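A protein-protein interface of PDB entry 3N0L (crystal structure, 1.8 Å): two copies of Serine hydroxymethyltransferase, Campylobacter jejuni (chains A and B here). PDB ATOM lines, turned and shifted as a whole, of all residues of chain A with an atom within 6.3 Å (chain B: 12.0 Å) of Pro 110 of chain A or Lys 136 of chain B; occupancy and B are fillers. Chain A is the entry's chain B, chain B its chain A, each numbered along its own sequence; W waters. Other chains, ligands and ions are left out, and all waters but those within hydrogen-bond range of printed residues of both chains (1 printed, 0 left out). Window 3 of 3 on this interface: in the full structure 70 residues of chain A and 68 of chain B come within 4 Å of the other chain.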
ATOM      1  N   TYR A 104      19.560  -6.782   0.535  1.00  0.00           N
ATOM      2  CA  TYR A 104      19.372  -5.414   1.049  1.00  0.00           C
ATOM      3  C   TYR A 104      17.977  -5.234   1.613  1.00  0.00           C
ATOM      4  O   TYR A 104      17.808  -4.743   2.728  1.00  0.00           O
ATOM      5  CB  TYR A 104      19.593  -4.368  -0.050  1.00  0.00           C
ATOM      6  CG  TYR A 104      20.995  -4.367  -0.597  1.00  0.00           C
ATOM      7  CD1 TYR A 104      22.063  -4.651   0.217  1.00  0.00           C
ATOM      8  CD2 TYR A 104      21.244  -4.100  -1.938  1.00  0.00           C
ATOM      9  CE1 TYR A 104      23.347  -4.659  -0.266  1.00  0.00           C
ATOM     10  CE2 TYR A 104      22.535  -4.115  -2.436  1.00  0.00           C
ATOM     11  CZ  TYR A 104      23.582  -4.396  -1.588  1.00  0.00           C
ATOM     12  OH  TYR A 104      24.879  -4.413  -2.046  1.00  0.00           O
ATOM     13  N   ALA A 105      16.978  -5.632   0.830  1.00  0.00           N
ATOM     14  CA  ALA A 105      15.580  -5.477   1.226  1.00  0.00           C
ATOM     15  C   ALA A 105      15.280  -6.287   2.485  1.00  0.00           C
ATOM     16  O   ALA A 105      14.452  -5.896   3.310  1.00  0.00           O
ATOM     17  CB  ALA A 105      14.652  -5.896   0.086  1.00  0.00           C
ATOM     18  N   ALA A 106      15.952  -7.422   2.630  1.00  0.00           N
ATOM     19  CA  ALA A 106      15.746  -8.275   3.797  1.00  0.00           C
ATOM     20  C   ALA A 106      16.352  -7.681   5.061  1.00  0.00           C
ATOM     21  O   ALA A 106      15.796  -7.840   6.146  1.00  0.00           O
ATOM     22  CB  ALA A 106      16.310  -9.679   3.550  1.00  0.00           C
ATOM     23  N   LEU A 107      17.485  -6.997   4.920  1.00  0.00           N
ATOM     24  CA  LEU A 107      18.312  -6.636   6.078  1.00  0.00           C
ATOM     25  C   LEU A 107      18.175  -5.185   6.524  1.00  0.00           C
ATOM     26  O   LEU A 107      18.298  -4.891   7.704  1.00  0.00           O
ATOM     27  CB  LEU A 107      19.784  -6.905   5.795  1.00  0.00           C
ATOM     28  CG  LEU A 107      20.163  -8.371   5.594  1.00  0.00           C
ATOM     29  CD1 LEU A 107      21.670  -8.504   5.515  1.00  0.00           C
ATOM     30  CD2 LEU A 107      19.597  -9.220   6.709  1.00  0.00           C
ATOM     31  N   ILE A 108      17.939  -4.277   5.584  1.00  0.00           N
ATOM     32  CA  ILE A 108      17.912  -2.855   5.921  1.00  0.00           C
ATOM     33  C   ILE A 108      16.722  -2.172   5.281  1.00  0.00           C
ATOM     34  O   ILE A 108      15.984  -2.785   4.522  1.00  0.00           O
ATOM     35  CB  ILE A 108      19.209  -2.141   5.498  1.00  0.00           C
ATOM     36  CG1 ILE A 108      19.319  -2.061   3.974  1.00  0.00           C
ATOM     37  CG2 ILE A 108      20.416  -2.850   6.092  1.00  0.00           C
ATOM     38  CD1 ILE A 108      20.646  -1.507   3.491  1.00  0.00           C
ATOM     39  N   ASN A 109      16.543  -0.898   5.599  1.00  0.00           N
ATOM     40  CA  ASN A 109      15.414  -0.128   5.083  1.00  0.00           C
ATOM     41  C   ASN A 109      15.840   0.873   4.017  1.00  0.00           C
ATOM     42  O   ASN A 109      16.995   1.301   3.989  1.00  0.00           O
ATOM     43  CB  ASN A 109      14.698   0.578   6.237  1.00  0.00           C
ATOM     44  CG  ASN A 109      14.074  -0.400   7.208  1.00  0.00           C
ATOM     45  OD1 ASN A 109      13.492  -1.405   6.800  1.00  0.00           O
ATOM     46  ND2 ASN A 109      14.205  -0.125   8.501  1.00  0.00           N
ATOM     47  N   PRO A 110      14.912   1.252   3.125  1.00  0.00           N
ATOM     48  CA  PRO A 110      15.288   2.250   2.124  1.00  0.00           C
ATOM     49  C   PRO A 110      15.890   3.464   2.816  1.00  0.00           C
ATOM     50  O   PRO A 110      15.401   3.854   3.873  1.00  0.00           O
ATOM     51  CB  PRO A 110      13.947   2.613   1.478  1.00  0.00           C
ATOM     52  CG  PRO A 110      13.109   1.379   1.657  1.00  0.00           C
ATOM     53  CD  PRO A 110      13.501   0.836   2.995  1.00  0.00           C
ATOM     54  N   GLY A 111      16.941   4.041   2.242  1.00  0.00           N
ATOM     55  CA  GLY A 111      17.585   5.195   2.846  1.00  0.00           C
ATOM     56  C   GLY A 111      18.738   4.835   3.772  1.00  0.00           C
ATOM     57  O   GLY A 111      19.601   5.674   4.040  1.00  0.00           O
ATOM     58  N   ASP A 112      18.761   3.600   4.273  1.00  0.00           N
ATOM     59  CA  ASP A 112      19.841   3.176   5.168  1.00  0.00           C
ATOM     60  C   ASP A 112      21.180   3.203   4.442  1.00  0.00           C
ATOM     61  O   ASP A 112      21.229   3.128   3.213  1.00  0.00           O
ATOM     62  CB  ASP A 112      19.602   1.763   5.725  1.00  0.00           C
ATOM     63  CG  ASP A 112      18.553   1.729   6.821  1.00  0.00           C
ATOM     64  OD1 ASP A 112      18.085   2.815   7.228  1.00  0.00           O
ATOM     65  OD2 ASP A 112      18.202   0.618   7.276  1.00  0.00           O
ATOM     66  N   MET A 137      18.033   4.434  -3.765  1.00  0.00           N
ATOM     67  CA  MET A 137      17.289   3.644  -2.780  1.00  0.00           C
ATOM     68  C   MET A 137      17.986   3.558  -1.416  1.00  0.00           C
ATOM     69  O   MET A 137      17.336   3.633  -0.373  1.00  0.00           O
ATOM     70  CB  MET A 137      17.029   2.237  -3.323  1.00  0.00           C
ATOM     71  CG  MET A 137      16.162   1.359  -2.425  1.00  0.00           C
ATOM     72  SD  MET A 137      14.421   2.153  -2.023  1.00  0.00           S
ATOM     73  CE  MET A 137      14.001   2.881  -3.778  1.00  0.00           C
ATOM     74  N   TYR A 138      19.306   3.389  -1.431  1.00  0.00           N
ATOM     75  CA  TYR A 138      20.089   3.363  -0.198  1.00  0.00           C
ATOM     76  C   TYR A 138      21.232   4.367  -0.276  1.00  0.00           C
ATOM     77  O   TYR A 138      21.627   4.783  -1.365  1.00  0.00           O
ATOM     78  CB  TYR A 138      20.668   1.954   0.046  1.00  0.00           C
ATOM     79  CG  TYR A 138      19.638   0.848   0.017  1.00  0.00           C
ATOM     80  CD1 TYR A 138      18.806   0.620   1.104  1.00  0.00           C
ATOM     81  CD2 TYR A 138      19.518   0.014  -1.088  1.00  0.00           C
ATOM     82  CE1 TYR A 138      17.864  -0.400   1.085  1.00  0.00           C
ATOM     83  CE2 TYR A 138      18.577  -0.999  -1.122  1.00  0.00           C
ATOM     84  CZ  TYR A 138      17.753  -1.202  -0.032  1.00  0.00           C
ATOM     85  OH  TYR A 138      16.822  -2.222  -0.061  1.00  0.00           O
ATOM     86  N   GLN B 101      10.182  -2.414 -12.346  1.00  0.00           N
ATOM     87  CA  GLN B 101      11.137  -1.688 -11.516  1.00  0.00           C
ATOM     88  C   GLN B 101      11.991  -0.715 -12.318  1.00  0.00           C
ATOM     89  O   GLN B 101      12.322   0.367 -11.832  1.00  0.00           O
ATOM     90  CB  GLN B 101      12.043  -2.676 -10.765  1.00  0.00           C
ATOM     91  CG  GLN B 101      11.276  -3.484  -9.743  1.00  0.00           C
ATOM     92  CD  GLN B 101      11.914  -4.832  -9.438  1.00  0.00           C
ATOM     93  OE1 GLN B 101      13.030  -5.131  -9.884  1.00  0.00           O
ATOM     94  NE2 GLN B 101      11.195  -5.658  -8.681  1.00  0.00           N
ATOM     95  N   TYR B 104       9.752   2.342 -13.060  1.00  0.00           N
ATOM     96  CA  TYR B 104       9.627   3.180 -11.869  1.00  0.00           C
ATOM     97  C   TYR B 104      10.915   3.970 -11.644  1.00  0.00           C
ATOM     98  O   TYR B 104      10.883   5.167 -11.369  1.00  0.00           O
ATOM     99  CB  TYR B 104       9.347   2.353 -10.612  1.00  0.00           C
ATOM    100  CG  TYR B 104       8.090   1.520 -10.668  1.00  0.00           C
ATOM    101  CD1 TYR B 104       6.993   1.944 -11.387  1.00  0.00           C
ATOM    102  CD2 TYR B 104       8.007   0.301 -10.001  1.00  0.00           C
ATOM    103  CE1 TYR B 104       5.847   1.190 -11.448  1.00  0.00           C
ATOM    104  CE2 TYR B 104       6.854  -0.465 -10.065  1.00  0.00           C
ATOM    105  CZ  TYR B 104       5.783  -0.009 -10.793  1.00  0.00           C
ATOM    106  OH  TYR B 104       4.626  -0.748 -10.867  1.00  0.00           O
ATOM    107  N   ILE B 108      10.325   8.096 -11.788  1.00  0.00           N
ATOM    108  CA  ILE B 108      10.014   8.742 -10.520  1.00  0.00           C
ATOM    109  C   ILE B 108      11.122   8.501  -9.505  1.00  0.00           C
ATOM    110  O   ILE B 108      12.069   7.756  -9.768  1.00  0.00           O
ATOM    111  CB  ILE B 108       8.654   8.254  -9.935  1.00  0.00           C
ATOM    112  CG1 ILE B 108       8.719   6.769  -9.578  1.00  0.00           C
ATOM    113  CG2 ILE B 108       7.484   8.534 -10.922  1.00  0.00           C
ATOM    114  CD1 ILE B 108       7.444   6.218  -8.937  1.00  0.00           C
ATOM    115  N   ASN B 109      10.989   9.126  -8.343  1.00  0.00           N
ATOM    116  CA  ASN B 109      11.979   9.004  -7.278  1.00  0.00           C
ATOM    117  C   ASN B 109      11.478   8.117  -6.143  1.00  0.00           C
ATOM    118  O   ASN B 109      10.271   8.024  -5.910  1.00  0.00           O
ATOM    119  CB  ASN B 109      12.316  10.390  -6.718  1.00  0.00           C
ATOM    120  CG  ASN B 109      12.883  11.324  -7.770  1.00  0.00           C
ATOM    121  OD1 ASN B 109      13.787  10.961  -8.522  1.00  0.00           O
ATOM    122  ND2 ASN B 109      12.345  12.537  -7.834  1.00  0.00           N
ATOM    123  N   PRO B 110      12.409   7.476  -5.415  1.00  0.00           N
ATOM    124  CA  PRO B 110      12.048   6.683  -4.237  1.00  0.00           C
ATOM    125  C   PRO B 110      11.136   7.506  -3.344  1.00  0.00           C
ATOM    126  O   PRO B 110      11.387   8.697  -3.167  1.00  0.00           O
ATOM    127  CB  PRO B 110      13.397   6.478  -3.529  1.00  0.00           C
ATOM    128  CG  PRO B 110      14.412   6.604  -4.598  1.00  0.00           C
ATOM    129  CD  PRO B 110      13.869   7.585  -5.592  1.00  0.00           C
ATOM    130  N   GLY B 111      10.091   6.896  -2.798  1.00  0.00           N
ATOM    131  CA  GLY B 111       9.160   7.631  -1.967  1.00  0.00           C
ATOM    132  C   GLY B 111       7.995   8.252  -2.722  1.00  0.00           C
ATOM    133  O   GLY B 111       6.952   8.522  -2.129  1.00  0.00           O
ATOM    134  N   ASP B 112       8.169   8.496  -4.021  1.00  0.00           N
ATOM    135  CA  ASP B 112       7.093   9.035  -4.856  1.00  0.00           C
ATOM    136  C   ASP B 112       5.877   8.115  -4.870  1.00  0.00           C
ATOM    137  O   ASP B 112       5.987   6.917  -4.619  1.00  0.00           O
ATOM    138  CB  ASP B 112       7.578   9.252  -6.295  1.00  0.00           C
ATOM    139  CG  ASP B 112       8.300  10.579  -6.482  1.00  0.00           C
ATOM    140  OD1 ASP B 112       8.370  11.378  -5.519  1.00  0.00           O
ATOM    141  OD2 ASP B 112       8.790  10.827  -7.606  1.00  0.00           O
ATOM    142  N   LYS B 113       4.716   8.667  -5.208  1.00  0.00           N
ATOM    143  CA  LYS B 113       3.480   7.905  -5.121  1.00  0.00           C
ATOM    144  C   LYS B 113       3.023   7.352  -6.476  1.00  0.00           C
ATOM    145  O   LYS B 113       3.051   8.059  -7.482  1.00  0.00           O
ATOM    146  CB  LYS B 113       2.391   8.786  -4.515  1.00  0.00           C
ATOM    147  CG  LYS B 113       1.044   8.110  -4.351  1.00  0.00           C
ATOM    148  CD  LYS B 113       0.004   9.107  -3.837  1.00  0.00           C
ATOM    149  CE  LYS B 113       0.451   9.763  -2.532  1.00  0.00           C
ATOM    150  NZ  LYS B 113      -0.619  10.619  -1.938  1.00  0.00           N
ATOM    151  N   ILE B 114       2.593   6.094  -6.473  1.00  0.00           N
ATOM    152  CA  ILE B 114       2.090   5.418  -7.662  1.00  0.00           C
ATOM    153  C   ILE B 114       0.630   5.008  -7.482  1.00  0.00           C
ATOM    154  O   ILE B 114       0.255   4.436  -6.456  1.00  0.00           O
ATOM    155  CB  ILE B 114       2.907   4.138  -7.936  1.00  0.00           C
ATOM    156  CG1 ILE B 114       4.384   4.457  -8.124  1.00  0.00           C
ATOM    157  CG2 ILE B 114       2.350   3.363  -9.136  1.00  0.00           C
ATOM    158  CD1 ILE B 114       5.266   3.202  -8.043  1.00  0.00           C
ATOM    159  N   LYS B 136       7.995  -0.890  -0.345  1.00  0.00           N
ATOM    160  CA  LYS B 136       8.799  -0.055   0.543  1.00  0.00           C
ATOM    161  C   LYS B 136       9.445   1.110  -0.197  1.00  0.00           C
ATOM    162  O   LYS B 136       9.618   2.190   0.364  1.00  0.00           O
ATOM    163  CB  LYS B 136       9.891  -0.885   1.225  1.00  0.00           C
ATOM    164  CG  LYS B 136       9.433  -1.685   2.429  1.00  0.00           C
ATOM    165  CD  LYS B 136      10.630  -2.289   3.145  1.00  0.00           C
ATOM    166  CE  LYS B 136      11.518  -3.060   2.173  1.00  0.00           C
ATOM    167  NZ  LYS B 136      12.735  -3.605   2.837  1.00  0.00           N
ATOM    168  N   MET B 137       9.810   0.881  -1.455  1.00  0.00           N
ATOM    169  CA  MET B 137      10.515   1.886  -2.246  1.00  0.00           C
ATOM    170  C   MET B 137       9.636   3.081  -2.617  1.00  0.00           C
ATOM    171  O   MET B 137      10.098   4.224  -2.607  1.00  0.00           O
ATOM    172  CB  MET B 137      11.104   1.252  -3.508  1.00  0.00           C
ATOM    173  N   TYR B 138       8.373   2.817  -2.932  1.00  0.00           N
ATOM    174  CA  TYR B 138       7.449   3.881  -3.345  1.00  0.00           C
ATOM    175  C   TYR B 138       6.159   3.831  -2.528  1.00  0.00           C
ATOM    176  O   TYR B 138       5.853   2.819  -1.909  1.00  0.00           O
ATOM    177  CB  TYR B 138       7.114   3.742  -4.831  1.00  0.00           C
ATOM    178  CG  TYR B 138       8.330   3.593  -5.714  1.00  0.00           C
ATOM    179  CD1 TYR B 138       9.112   4.690  -6.040  1.00  0.00           C
ATOM    180  CD2 TYR B 138       8.701   2.356  -6.209  1.00  0.00           C
ATOM    181  CE1 TYR B 138      10.232   4.558  -6.844  1.00  0.00           C
ATOM    182  CE2 TYR B 138       9.813   2.215  -7.014  1.00  0.00           C
ATOM    183  CZ  TYR B 138      10.575   3.321  -7.329  1.00  0.00           C
ATOM    184  OH  TYR B 138      11.689   3.191  -8.127  1.00  0.00           O
ATOM    185  N   GLU B 139       5.398   4.918  -2.516  1.00  0.00           N
ATOM    186  CA  GLU B 139       4.075   4.850  -1.908  1.00  0.00           C
ATOM    187  C   GLU B 139       3.069   4.379  -2.952  1.00  0.00           C
ATOM    188  O   GLU B 139       3.121   4.815  -4.103  1.00  0.00           O
ATOM    189  CB  GLU B 139       3.651   6.193  -1.321  1.00  0.00           C
ATOM    190  CG  GLU B 139       2.307   6.115  -0.603  1.00  0.00           C
ATOM    191  CD  GLU B 139       1.822   7.459  -0.092  1.00  0.00           C
ATOM    192  OE1 GLU B 139       2.665   8.362   0.103  1.00  0.00           O
ATOM    193  OE2 GLU B 139       0.596   7.611   0.107  1.00  0.00           O
ATOM    194  N   SER B 140       2.169   3.485  -2.549  1.00  0.00           N
ATOM    195  CA  SER B 140       1.186   2.907  -3.461  1.00  0.00           C
ATOM    196  C   SER B 140      -0.253   3.266  -3.104  1.00  0.00           C
ATOM    197  O   SER B 140      -0.647   3.197  -1.940  1.00  0.00           O
ATOM    198  CB  SER B 140       1.311   1.384  -3.459  1.00  0.00           C
ATOM    199  OG  SER B 140       2.505   0.961  -4.094  1.00  0.00           O
ATOM    200  N   CYS B 141      -1.028   3.666  -4.109  1.00  0.00           N
ATOM    201  CA  CYS B 141      -2.465   3.889  -3.971  1.00  0.00           C
ATOM    202  C   CYS B 141      -3.187   3.116  -5.072  1.00  0.00           C
ATOM    203  O   CYS B 141      -2.573   2.776  -6.086  1.00  0.00           O
ATOM    204  CB  CYS B 141      -2.800   5.376  -4.087  1.00  0.00           C
ATOM    205  SG  CYS B 141      -2.029   6.410  -2.831  1.00  0.00           S
ATOM    206  N   PHE B 142      -4.483   2.858  -4.893  1.00  0.00           N
ATOM    207  CA  PHE B 142      -5.189   1.987  -5.834  1.00  0.00           C
ATOM    208  C   PHE B 142      -6.546   2.463  -6.314  1.00  0.00           C
ATOM    209  O   PHE B 142      -7.263   3.167  -5.609  1.00  0.00           O
ATOM    210  CB  PHE B 142      -5.379   0.598  -5.226  1.00  0.00           C
ATOM    211  CG  PHE B 142      -4.091  -0.056  -4.801  1.00  0.00           C
ATOM    212  CD1 PHE B 142      -3.385  -0.861  -5.679  1.00  0.00           C
ATOM    213  CD2 PHE B 142      -3.586   0.149  -3.528  1.00  0.00           C
ATOM    214  CE1 PHE B 142      -2.200  -1.463  -5.290  1.00  0.00           C
ATOM    215  CE2 PHE B 142      -2.399  -0.447  -3.137  1.00  0.00           C
ATOM    216  CZ  PHE B 142      -1.709  -1.254  -4.024  1.00  0.00           C
HETATM  217  O   HOH W   1      15.101  -2.137   1.903  1.00  0.00           O
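Met 137 of chain A touches Pro 110 of chain B, but with the chains exchanged Pro 110 of chain A does not touch Met 137 of chain B (4.6 Å).
Met 137 of chain A touches its own counterpart, Met 137 of chain B.
Positions printed for both chains: 104, 108, 109, 110, 111, 112, 137 and 138.
Of the 5 pairs that touch across the chains among the printed residues, 1 has its exchanged pair printed and touching as well.
The side-chain amino group (NZ) of Lys 136 of chain B is in hydrogen-bond range of the backbone carbonyl oxygen (O) of Ala 105 of chain A (2.9 Å).
Of the 16 printed residues of chain B, 3 touch a printed residue of chain A.
Hydrophobic or aromatic side chains of chain B that line the printed part of chain A: Pro 110 and Met 137.
Along chain A the printed residues that touch a printed residue of chain B span positions 105 to 137.
Water W1 lies within hydrogen-bond range of the side-chain hydroxyl (OH) of Tyr 138 of chain A, the backbone carbonyl oxygen (O) of Ile 108 of chain A and the side-chain amino group (NZ) of Lys 136 of chain B.
O of Met 137 of chain B is in hydrogen-bond range of N of Gly 111 of chain B, at 2.7 Å.
The backbone carbonyl oxygen of Met 137 of chain A is in hydrogen-bond range of the backbone NH of Gly 111 of chain A, at 2.7 Å.
O of Ile 108 of chain A touches NZ of Lys 136 of chain B (3.8 Å).
CG of Pro 110 of chain A touches O of Lys 136 of chain B, at 3.8 Å.
CE of Met 137 of chain A touches CB of Pro 110 of chain B (3.7 Å).
CE of Met 137 of chain A touches CB of Met 137 of chain B, 3.3 Å away.
Of chain B, only Lys 136 comes within 4 Å of Pro 110 of chain A.
Of the printed residues of chain A, Lys 136 of chain B touches Ala 105 (2.9 Å), Ile 108 (3.8 Å) and Pro 110 (3.8 Å).
Ala 105 of chain A touches one residue of chain B.
Ala 106 of chain A touches none of the printed residues of chain B.
Of chain B, only Lys 136 (3.8 Å) comes within 4 Å of Ile 108 of chain A.
No residue of chain B comes within 4 Å of Asn 109 of chain A.
No residue of chain B comes within 4 Å of Gly 111 of chain A.
No residue of chain B comes within 4 Å of Asp 112 of chain A.
Met 137 of chain A touches just these residues of chain B: Pro 110 (3.7 Å) and Met 137 (3.3 Å).
No residue of chain B comes within 4 Å of Tyr 138 of chain A.
Of the printed residues of chain A, Met 137 of chain B touches Met 137 (3.3 Å).
Of the printed residues of chain A, Pro 110 of chain B touches Met 137 (3.7 Å).
The nearest residue of chain B that does not touch Pro 110 of chain A is Met 137 of chain B (4.6 Å).
The nearest residue of chain A that does not touch Lys 136 of chain B is Asn 109 of chain A (4.6 Å).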
